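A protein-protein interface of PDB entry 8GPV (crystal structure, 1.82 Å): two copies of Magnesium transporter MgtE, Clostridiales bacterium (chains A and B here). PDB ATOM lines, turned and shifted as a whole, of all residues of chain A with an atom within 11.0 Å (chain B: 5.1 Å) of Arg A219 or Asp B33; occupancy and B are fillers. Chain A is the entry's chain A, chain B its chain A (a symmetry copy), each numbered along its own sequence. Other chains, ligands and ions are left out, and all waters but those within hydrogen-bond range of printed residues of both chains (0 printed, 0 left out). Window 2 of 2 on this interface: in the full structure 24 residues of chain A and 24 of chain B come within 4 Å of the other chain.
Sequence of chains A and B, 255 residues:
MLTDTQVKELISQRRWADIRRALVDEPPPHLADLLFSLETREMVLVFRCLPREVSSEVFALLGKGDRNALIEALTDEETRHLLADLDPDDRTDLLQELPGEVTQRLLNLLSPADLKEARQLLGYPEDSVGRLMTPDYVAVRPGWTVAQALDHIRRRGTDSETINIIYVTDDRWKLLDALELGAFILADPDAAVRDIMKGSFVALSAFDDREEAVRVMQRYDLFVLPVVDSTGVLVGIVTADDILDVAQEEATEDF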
ATOM      1  N   PHE A 201      24.856  10.645  19.579  1.00  0.00           N
ATOM      2  CA  PHE A 201      25.320  10.948  20.924  1.00  0.00           C
ATOM      3  C   PHE A 201      24.890  12.361  21.282  1.00  0.00           C
ATOM      4  O   PHE A 201      24.567  13.172  20.411  1.00  0.00           O
ATOM      5  CB  PHE A 201      26.835  10.805  21.044  1.00  0.00           C
ATOM      6  CG  PHE A 201      27.612  11.682  20.102  1.00  0.00           C
ATOM      7  CD1 PHE A 201      27.921  13.000  20.438  1.00  0.00           C
ATOM      8  CD2 PHE A 201      28.071  11.180  18.899  1.00  0.00           C
ATOM      9  CE1 PHE A 201      28.627  13.814  19.566  1.00  0.00           C
ATOM     10  CE2 PHE A 201      28.786  11.985  18.025  1.00  0.00           C
ATOM     11  CZ  PHE A 201      29.070  13.303  18.363  1.00  0.00           C
ATOM     12  N   VAL A 202      24.857  12.628  22.573  1.00  0.00           N
ATOM     13  CA  VAL A 202      24.656  13.979  23.081  1.00  0.00           C
ATOM     14  C   VAL A 202      26.000  14.522  23.513  1.00  0.00           C
ATOM     15  O   VAL A 202      26.783  13.815  24.164  1.00  0.00           O
ATOM     16  CB  VAL A 202      23.673  14.005  24.264  1.00  0.00           C
ATOM     17  CG1 VAL A 202      23.311  15.438  24.599  1.00  0.00           C
ATOM     18  CG2 VAL A 202      22.423  13.213  23.915  1.00  0.00           C
ATOM     19  N   ALA A 203      26.251  15.790  23.216  1.00  0.00           N
ATOM     20  CA  ALA A 203      27.472  16.419  23.711  1.00  0.00           C
ATOM     21  C   ALA A 203      27.190  17.868  24.072  1.00  0.00           C
ATOM     22  O   ALA A 203      26.293  18.512  23.517  1.00  0.00           O
ATOM     23  CB  ALA A 203      28.625  16.343  22.709  1.00  0.00           C
ATOM     24  N   LEU A 204      27.957  18.363  25.026  1.00  0.00           N
ATOM     25  CA  LEU A 204      27.895  19.751  25.433  1.00  0.00           C
ATOM     26  C   LEU A 204      28.976  20.544  24.714  1.00  0.00           C
ATOM     27  O   LEU A 204      29.954  19.995  24.185  1.00  0.00           O
ATOM     28  CB  LEU A 204      28.086  19.867  26.948  1.00  0.00           C
ATOM     29  CG  LEU A 204      27.016  19.301  27.869  1.00  0.00           C
ATOM     30  CD1 LEU A 204      27.586  19.248  29.294  1.00  0.00           C
ATOM     31  CD2 LEU A 204      25.755  20.136  27.829  1.00  0.00           C
ATOM     32  N   GLU A 211      24.583  25.523  34.014  1.00  0.00           N
ATOM     33  CA  GLU A 211      23.197  25.099  34.167  1.00  0.00           C
ATOM     34  C   GLU A 211      22.696  24.338  32.950  1.00  0.00           C
ATOM     35  O   GLU A 211      21.724  23.579  33.062  1.00  0.00           O
ATOM     36  CB  GLU A 211      22.305  26.312  34.408  1.00  0.00           C
ATOM     37  CG  GLU A 211      22.633  27.032  35.691  1.00  0.00           C
ATOM     38  CD  GLU A 211      21.485  27.856  36.222  1.00  0.00           C
ATOM     39  OE1 GLU A 211      21.585  29.101  36.146  1.00  0.00           O
ATOM     40  OE2 GLU A 211      20.514  27.270  36.752  1.00  0.00           O
ATOM     41  N   GLU A 212      23.320  24.538  31.789  1.00  0.00           N
ATOM     42  CA  GLU A 212      22.936  23.744  30.628  1.00  0.00           C
ATOM     43  C   GLU A 212      23.360  22.292  30.812  1.00  0.00           C
ATOM     44  O   GLU A 212      22.631  21.371  30.412  1.00  0.00           O
ATOM     45  CB  GLU A 212      23.539  24.347  29.354  1.00  0.00           C
ATOM     46  CG  GLU A 212      23.285  23.537  28.066  1.00  0.00           C
ATOM     47  CD  GLU A 212      21.874  23.732  27.512  1.00  0.00           C
ATOM     48  OE1 GLU A 212      21.085  24.474  28.142  1.00  0.00           O
ATOM     49  OE2 GLU A 212      21.554  23.148  26.446  1.00  0.00           O
ATOM     50  N   ALA A 213      24.538  22.072  31.419  1.00  0.00           N
ATOM     51  CA  ALA A 213      24.946  20.721  31.806  1.00  0.00           C
ATOM     52  C   ALA A 213      23.882  20.060  32.665  1.00  0.00           C
ATOM     53  O   ALA A 213      23.549  18.885  32.466  1.00  0.00           O
ATOM     54  CB  ALA A 213      26.288  20.752  32.549  1.00  0.00           C
ATOM     55  N   VAL A 214      23.316  20.805  33.619  1.00  0.00           N
ATOM     56  CA  VAL A 214      22.224  20.258  34.420  1.00  0.00           C
ATOM     57  C   VAL A 214      21.017  19.942  33.545  1.00  0.00           C
ATOM     58  O   VAL A 214      20.419  18.870  33.663  1.00  0.00           O
ATOM     59  CB  VAL A 214      21.846  21.215  35.563  1.00  0.00           C
ATOM     60  CG1 VAL A 214      20.782  20.577  36.406  1.00  0.00           C
ATOM     61  CG2 VAL A 214      23.054  21.507  36.430  1.00  0.00           C
ATOM     62  N   ARG A 215      20.611  20.881  32.685  1.00  0.00           N
ATOM     63  CA  ARG A 215      19.415  20.632  31.876  1.00  0.00           C
ATOM     64  C   ARG A 215      19.627  19.446  30.939  1.00  0.00           C
ATOM     65  O   ARG A 215      18.748  18.589  30.799  1.00  0.00           O
ATOM     66  CB  ARG A 215      19.021  21.884  31.086  1.00  0.00           C
ATOM     67  CG  ARG A 215      17.760  21.689  30.191  1.00  0.00           C
ATOM     68  CD  ARG A 215      17.487  22.913  29.301  1.00  0.00           C
ATOM     69  NE  ARG A 215      18.317  22.907  28.092  1.00  0.00           N
ATOM     70  CZ  ARG A 215      18.254  21.999  27.116  1.00  0.00           C
ATOM     71  NH1 ARG A 215      17.350  21.022  27.152  1.00  0.00           N
ATOM     72  NH2 ARG A 215      19.077  22.093  26.075  1.00  0.00           N
ATOM     73  N   VAL A 216      20.810  19.352  30.320  1.00  0.00           N
ATOM     74  CA  VAL A 216      21.036  18.272  29.364  1.00  0.00           C
ATOM     75  C   VAL A 216      21.144  16.931  30.081  1.00  0.00           C
ATOM     76  O   VAL A 216      20.607  15.916  29.618  1.00  0.00           O
ATOM     77  CB  VAL A 216      22.269  18.587  28.501  1.00  0.00           C
ATOM     78  CG1 VAL A 216      22.673  17.378  27.650  1.00  0.00           C
ATOM     79  CG2 VAL A 216      21.976  19.814  27.615  1.00  0.00           C
ATOM     80  N   MET A 217      21.809  16.908  31.240  1.00  0.00           N
ATOM     81  CA  MET A 217      21.906  15.665  31.999  1.00  0.00           C
ATOM     82  C   MET A 217      20.544  15.175  32.487  1.00  0.00           C
ATOM     83  O   MET A 217      20.285  13.962  32.487  1.00  0.00           O
ATOM     84  CB  MET A 217      22.869  15.850  33.180  1.00  0.00           C
ATOM     85  CG  MET A 217      23.100  14.573  33.933  1.00  0.00           C
ATOM     86  SD  MET A 217      24.742  14.494  34.680  1.00  0.00           S
ATOM     87  CE  MET A 217      25.749  14.167  33.239  1.00  0.00           C
ATOM     88  N   GLN A 218      19.663  16.083  32.950  1.00  0.00           N
ATOM     89  CA  GLN A 218      18.299  15.657  33.287  1.00  0.00           C
ATOM     90  C   GLN A 218      17.545  15.147  32.073  1.00  0.00           C
ATOM     91  O   GLN A 218      16.749  14.200  32.176  1.00  0.00           O
ATOM     92  CB  GLN A 218      17.457  16.775  33.917  1.00  0.00           C
ATOM     93  CG  GLN A 218      17.529  16.840  35.436  1.00  0.00           C
ATOM     94  CD  GLN A 218      16.662  17.950  36.042  1.00  0.00           C
ATOM     95  OE1 GLN A 218      15.686  17.668  36.748  1.00  0.00           O
ATOM     96  NE2 GLN A 218      16.995  19.201  35.749  1.00  0.00           N
ATOM     97  N   ARG A 219      17.732  15.799  30.931  1.00  0.00           N
ATOM     98  CA  ARG A 219      16.944  15.466  29.747  1.00  0.00           C
ATOM     99  C   ARG A 219      17.223  14.045  29.258  1.00  0.00           C
ATOM    100  O   ARG A 219      16.293  13.305  28.904  1.00  0.00           O
ATOM    101  CB  ARG A 219      17.240  16.485  28.649  1.00  0.00           C
ATOM    102  CG  ARG A 219      16.324  16.410  27.448  1.00  0.00           C
ATOM    103  CD  ARG A 219      16.582  17.614  26.567  1.00  0.00           C
ATOM    104  NE  ARG A 219      16.240  17.352  25.178  1.00  0.00           N
ATOM    105  CZ  ARG A 219      15.001  17.431  24.717  1.00  0.00           C
ATOM    106  NH1 ARG A 219      14.016  17.728  25.558  1.00  0.00           N
ATOM    107  NH2 ARG A 219      14.739  17.194  23.439  1.00  0.00           N
ATOM    108  N   TYR A 220      18.494  13.652  29.205  1.00  0.00           N
ATOM    109  CA  TYR A 220      18.883  12.376  28.616  1.00  0.00           C
ATOM    110  C   TYR A 220      19.220  11.302  29.645  1.00  0.00           C
ATOM    111  O   TYR A 220      19.574  10.184  29.257  1.00  0.00           O
ATOM    112  CB  TYR A 220      20.061  12.581  27.646  1.00  0.00           C
ATOM    113  CG  TYR A 220      19.706  13.502  26.488  1.00  0.00           C
ATOM    114  CD1 TYR A 220      19.038  13.013  25.374  1.00  0.00           C
ATOM    115  CD2 TYR A 220      20.049  14.862  26.503  1.00  0.00           C
ATOM    116  CE1 TYR A 220      18.682  13.845  24.315  1.00  0.00           C
ATOM    117  CE2 TYR A 220      19.698  15.714  25.427  1.00  0.00           C
ATOM    118  CZ  TYR A 220      19.018  15.186  24.333  1.00  0.00           C
ATOM    119  OH  TYR A 220      18.643  15.978  23.250  1.00  0.00           O
ATOM    120  N   ASP A 221      19.144  11.620  30.937  1.00  0.00           N
ATOM    121  CA  ASP A 221      19.326  10.653  32.023  1.00  0.00           C
ATOM    122  C   ASP A 221      20.628   9.870  31.872  1.00  0.00           C
ATOM    123  O   ASP A 221      20.652   8.637  31.897  1.00  0.00           O
ATOM    124  CB  ASP A 221      18.125   9.715  32.121  1.00  0.00           C
ATOM    125  CG  ASP A 221      16.840  10.468  32.288  1.00  0.00           C
ATOM    126  OD1 ASP A 221      16.843  11.425  33.092  1.00  0.00           O
ATOM    127  OD2 ASP A 221      15.833  10.113  31.620  1.00  0.00           O
ATOM    128  N   LEU A 222      21.726  10.608  31.717  1.00  0.00           N
ATOM    129  CA  LEU A 222      23.058  10.044  31.577  1.00  0.00           C
ATOM    130  C   LEU A 222      23.860  10.429  32.807  1.00  0.00           C
ATOM    131  O   LEU A 222      23.571  11.450  33.436  1.00  0.00           O
ATOM    132  CB  LEU A 222      23.769  10.594  30.333  1.00  0.00           C
ATOM    133  CG  LEU A 222      23.141  10.211  29.006  1.00  0.00           C
ATOM    134  CD1 LEU A 222      23.894  10.907  27.887  1.00  0.00           C
ATOM    135  CD2 LEU A 222      23.177   8.693  28.847  1.00  0.00           C
ATOM    136  N   PHE A 223      24.860   9.606  33.154  1.00  0.00           N
ATOM    137  CA  PHE A 223      25.719   9.931  34.299  1.00  0.00           C
ATOM    138  C   PHE A 223      26.996  10.666  33.897  1.00  0.00           C
ATOM    139  O   PHE A 223      27.709  11.160  34.780  1.00  0.00           O
ATOM    140  CB  PHE A 223      26.127   8.670  35.069  1.00  0.00           C
ATOM    141  CG  PHE A 223      24.974   7.851  35.554  1.00  0.00           C
ATOM    142  CD1 PHE A 223      23.752   8.445  35.831  1.00  0.00           C
ATOM    143  CD2 PHE A 223      25.118   6.485  35.748  1.00  0.00           C
ATOM    144  CE1 PHE A 223      22.676   7.685  36.272  1.00  0.00           C
ATOM    145  CE2 PHE A 223      24.043   5.717  36.199  1.00  0.00           C
ATOM    146  CZ  PHE A 223      22.830   6.324  36.463  1.00  0.00           C
ATOM    147  N   VAL A 224      27.330  10.704  32.609  1.00  0.00           N
ATOM    148  CA  VAL A 224      28.508  11.421  32.107  1.00  0.00           C
ATOM    149  C   VAL A 224      28.140  12.049  30.768  1.00  0.00           C
ATOM    150  O   VAL A 224      27.364  11.486  29.991  1.00  0.00           O
ATOM    151  CB  VAL A 224      29.727  10.469  31.980  1.00  0.00           C
ATOM    152  CG1 VAL A 224      29.414   9.402  31.051  1.00  0.00           C
ATOM    153  CG2 VAL A 224      31.032  11.192  31.494  1.00  0.00           C
ATOM    154  N   LEU A 225      28.677  13.231  30.504  1.00  0.00           N
ATOM    155  CA  LEU A 225      28.422  13.889  29.236  1.00  0.00           C
ATOM    156  C   LEU A 225      29.755  14.321  28.643  1.00  0.00           C
ATOM    157  O   LEU A 225      30.616  14.848  29.363  1.00  0.00           O
ATOM    158  CB  LEU A 225      27.512  15.112  29.378  1.00  0.00           C
ATOM    159  CG  LEU A 225      26.018  14.936  29.662  1.00  0.00           C
ATOM    160  CD1 LEU A 225      25.394  16.317  29.928  1.00  0.00           C
ATOM    161  CD2 LEU A 225      25.345  14.229  28.511  1.00  0.00           C
ATOM    162  N   ILE A 243      27.537  17.605  38.615  1.00  0.00           N
ATOM    163  CA  ILE A 243      26.341  18.280  38.116  1.00  0.00           C
ATOM    164  C   ILE A 243      25.298  18.399  39.219  1.00  0.00           C
ATOM    165  O   ILE A 243      24.577  19.400  39.311  1.00  0.00           O
ATOM    166  CB  ILE A 243      25.789  17.547  36.876  1.00  0.00           C
ATOM    167  CG1 ILE A 243      26.813  17.583  35.728  1.00  0.00           C
ATOM    168  CG2 ILE A 243      24.469  18.135  36.453  1.00  0.00           C
ATOM    169  CD1 ILE A 243      27.425  18.950  35.445  1.00  0.00           C
ATOM    170  N   PRO B  28      14.174   9.208  22.829  1.00  0.00           N
ATOM    171  CA  PRO B  28      12.917   9.365  23.565  1.00  0.00           C
ATOM    172  C   PRO B  28      12.656  10.803  23.991  1.00  0.00           C
ATOM    173  O   PRO B  28      11.505  11.256  23.926  1.00  0.00           O
ATOM    174  CB  PRO B  28      13.123   8.438  24.770  1.00  0.00           C
ATOM    175  CG  PRO B  28      13.932   7.298  24.147  1.00  0.00           C
ATOM    176  CD  PRO B  28      14.937   8.036  23.288  1.00  0.00           C
ATOM    177  N   PRO B  29      13.661  11.561  24.465  1.00  0.00           N
ATOM    178  CA  PRO B  29      13.376  12.971  24.796  1.00  0.00           C
ATOM    179  C   PRO B  29      12.888  13.773  23.602  1.00  0.00           C
ATOM    180  O   PRO B  29      12.058  14.682  23.758  1.00  0.00           O
ATOM    181  CB  PRO B  29      14.737  13.495  25.290  1.00  0.00           C
ATOM    182  CG  PRO B  29      15.409  12.271  25.830  1.00  0.00           C
ATOM    183  CD  PRO B  29      15.055  11.221  24.804  1.00  0.00           C
ATOM    184  N   HIS B  30      13.396  13.468  22.410  1.00  0.00           N
ATOM    185  CA  HIS B  30      12.944  14.176  21.220  1.00  0.00           C
ATOM    186  C   HIS B  30      11.513  13.774  20.868  1.00  0.00           C
ATOM    187  O   HIS B  30      10.714  14.620  20.450  1.00  0.00           O
ATOM    188  CB  HIS B  30      13.871  13.886  20.040  1.00  0.00           C
ATOM    189  CG  HIS B  30      15.276  14.397  20.205  1.00  0.00           C
ATOM    190  ND1 HIS B  30      16.190  14.390  19.171  1.00  0.00           N
ATOM    191  CD2 HIS B  30      15.951  14.846  21.295  1.00  0.00           C
ATOM    192  CE1 HIS B  30      17.347  14.864  19.598  1.00  0.00           C
ATOM    193  NE2 HIS B  30      17.232  15.142  20.886  1.00  0.00           N
ATOM    194  N   LEU B  31      11.166  12.483  21.029  1.00  0.00           N
ATOM    195  CA  LEU B  31       9.781  12.068  20.832  1.00  0.00           C
ATOM    196  C   LEU B  31       8.868  12.717  21.855  1.00  0.00           C
ATOM    197  O   LEU B  31       7.735  13.089  21.533  1.00  0.00           O
ATOM    198  CB  LEU B  31       9.647  10.543  20.916  1.00  0.00           C
ATOM    199  CG  LEU B  31      10.325   9.841  19.751  1.00  0.00           C
ATOM    200  CD1 LEU B  31      10.464   8.360  20.044  1.00  0.00           C
ATOM    201  CD2 LEU B  31       9.568  10.082  18.433  1.00  0.00           C
ATOM    202  N   ALA B  32       9.332  12.833  23.108  1.00  0.00           N
ATOM    203  CA  ALA B  32       8.526  13.495  24.124  1.00  0.00           C
ATOM    204  C   ALA B  32       8.310  14.960  23.778  1.00  0.00           C
ATOM    205  O   ALA B  32       7.239  15.512  24.059  1.00  0.00           O
ATOM    206  CB  ALA B  32       9.184  13.377  25.507  1.00  0.00           C
ATOM    207  N   ASP B  33       9.307  15.609  23.177  1.00  0.00           N
ATOM    208  CA  ASP B  33       9.115  17.003  22.790  1.00  0.00           C
ATOM    209  C   ASP B  33       8.057  17.120  21.705  1.00  0.00           C
ATOM    210  O   ASP B  33       7.163  17.969  21.785  1.00  0.00           O
ATOM    211  CB  ASP B  33      10.431  17.630  22.336  1.00  0.00           C
ATOM    212  CG  ASP B  33      11.369  17.898  23.497  1.00  0.00           C
ATOM    213  OD1 ASP B  33      10.867  17.996  24.632  1.00  0.00           O
ATOM    214  OD2 ASP B  33      12.586  18.035  23.271  1.00  0.00           O
ATOM    215  N   LEU B  34       8.136  16.252  20.696  1.00  0.00           N
ATOM    216  CA  LEU B  34       7.149  16.244  19.620  1.00  0.00           C
ATOM    217  C   LEU B  34       5.748  15.995  20.157  1.00  0.00           C
ATOM    218  O   LEU B  34       4.791  16.671  19.767  1.00  0.00           O
ATOM    219  CB  LEU B  34       7.529  15.183  18.586  1.00  0.00           C
ATOM    220  CG  LEU B  34       6.520  14.934  17.460  1.00  0.00           C
ATOM    221  CD1 LEU B  34       6.531  16.141  16.548  1.00  0.00           C
ATOM    222  CD2 LEU B  34       6.881  13.670  16.695  1.00  0.00           C
ATOM    223  N   LEU B  35       5.598  15.005  21.037  1.00  0.00           N
ATOM    224  CA  LEU B  35       4.276  14.712  21.582  1.00  0.00           C
ATOM    225  C   LEU B  35       3.727  15.897  22.366  1.00  0.00           C
ATOM    226  O   LEU B  35       2.519  16.161  22.338  1.00  0.00           O
ATOM    227  CB  LEU B  35       4.337  13.458  22.448  1.00  0.00           C
ATOM    228  CG  LEU B  35       3.955  12.154  21.745  1.00  0.00           C
ATOM    229  CD1 LEU B  35       4.993  11.766  20.730  1.00  0.00           C
ATOM    230  CD2 LEU B  35       3.821  11.044  22.776  1.00  0.00           C
ATOM    231  N   PHE B  36       4.598  16.634  23.064  1.00  0.00           N
ATOM    232  CA  PHE B  36       4.127  17.799  23.812  1.00  0.00           C
ATOM    233  C   PHE B  36       3.623  18.894  22.877  1.00  0.00           C
ATOM    234  O   PHE B  36       2.569  19.495  23.122  1.00  0.00           O
ATOM    235  CB  PHE B  36       5.238  18.349  24.704  1.00  0.00           C
ATOM    236  CG  PHE B  36       4.906  19.682  25.320  1.00  0.00           C
ATOM    237  CD1 PHE B  36       3.899  19.786  26.275  1.00  0.00           C
ATOM    238  CD2 PHE B  36       5.596  20.826  24.945  1.00  0.00           C
ATOM    239  CE1 PHE B  36       3.584  21.006  26.844  1.00  0.00           C
ATOM    240  CE2 PHE B  36       5.292  22.059  25.512  1.00  0.00           C
ATOM    241  CZ  PHE B  36       4.284  22.148  26.464  1.00  0.00           C
ATOM    242  N   SER B  37       4.377  19.179  21.810  1.00  0.00           N
ATOM    243  CA  SER B  37       4.032  20.244  20.874  1.00  0.00           C
ATOM    244  C   SER B  37       2.793  19.925  20.058  1.00  0.00           C
ATOM    245  O   SER B  37       2.270  20.821  19.386  1.00  0.00           O
ATOM    246  CB  SER B  37       5.202  20.531  19.926  1.00  0.00           C
ATOM    247  OG  SER B  37       5.294  19.568  18.886  1.00  0.00           O
ATOM    248  N   LEU B  61       8.759  10.335  30.222  1.00  0.00           N
ATOM    249  CA  LEU B  61       9.316  11.665  30.028  1.00  0.00           C
ATOM    250  C   LEU B  61       8.258  12.749  29.857  1.00  0.00           C
ATOM    251  O   LEU B  61       8.601  13.938  29.877  1.00  0.00           O
ATOM    252  CB  LEU B  61      10.241  11.678  28.806  1.00  0.00           C
ATOM    253  CG  LEU B  61      11.402  10.701  28.863  1.00  0.00           C
ATOM    254  CD1 LEU B  61      12.171  10.700  27.544  1.00  0.00           C
ATOM    255  CD2 LEU B  61      12.317  11.058  30.013  1.00  0.00           C
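OH of Tyr A220 sits at hydrogen-bond distance from NE2 of His B30, 2.9 Å away.
The side-chain carboxylate (OD2) of Asp B33 is in salt-bridge range of the guanidinium group (NH1) of Arg A219 (2.7 Å).
The guanidinium group (NE) of Arg A219 lies within hydrogen-bond range of the side-chain hydroxyl (OH) of Tyr A220 (3.4 Å).
Among the printed residues, merely in contact across the chains: Arg A219 with Pro B29 (3.4 Å), Arg A219 with His B30 (3.4 Å), Tyr A220 with Pro B29 (3.7 Å) and Asp A221 with Leu B61 (3.98 Å).
Arg A219 touches just these residues of chain B: Pro B29 (3.4 Å), His B30 (3.4 Å) and Asp B33 (2.3 Å).
Asp B33 touches just one residue of chain A: Arg A219 (2.3 Å).
Pro B29 touches two residues of chain A.
No residue of chain A comes within 4 Å of Ala B32.
No residue of chain A comes within 4 Å of Phe B36.
Of the printed residues of chain B, Tyr A220 touches Pro B29 (3.7 Å) and His B30 (2.9 Å).
Printed residues of chain A within 4 Å of Leu B61: Asp A221 (3.98 Å).
Of the printed residues of chain B, Asp A221 touches Leu B61 (3.98 Å).
Leu B31 touches none of the printed residues of chain A.
The nearest residue of chain B that does not touch Arg A219 is Leu B61 (4.7 Å).
Printed residues of chain A that touch a printed residue of chain B: Arg A219, Tyr A220 and Asp A221.
Hydrophobic or aromatic side chains of chain A that line the printed part of chain B: Tyr A220.
Among the printed residues, Asp or Glu carboxylates within 4 Å of a Lys or Arg side-chain nitrogen of the other chain: Arg A219 with Asp B33 (2.3 Å).
No position is printed for both chains.
Of the 6 pairs that touch across the chains among the printed residues, none has its exchanged pair printed and touching as well.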
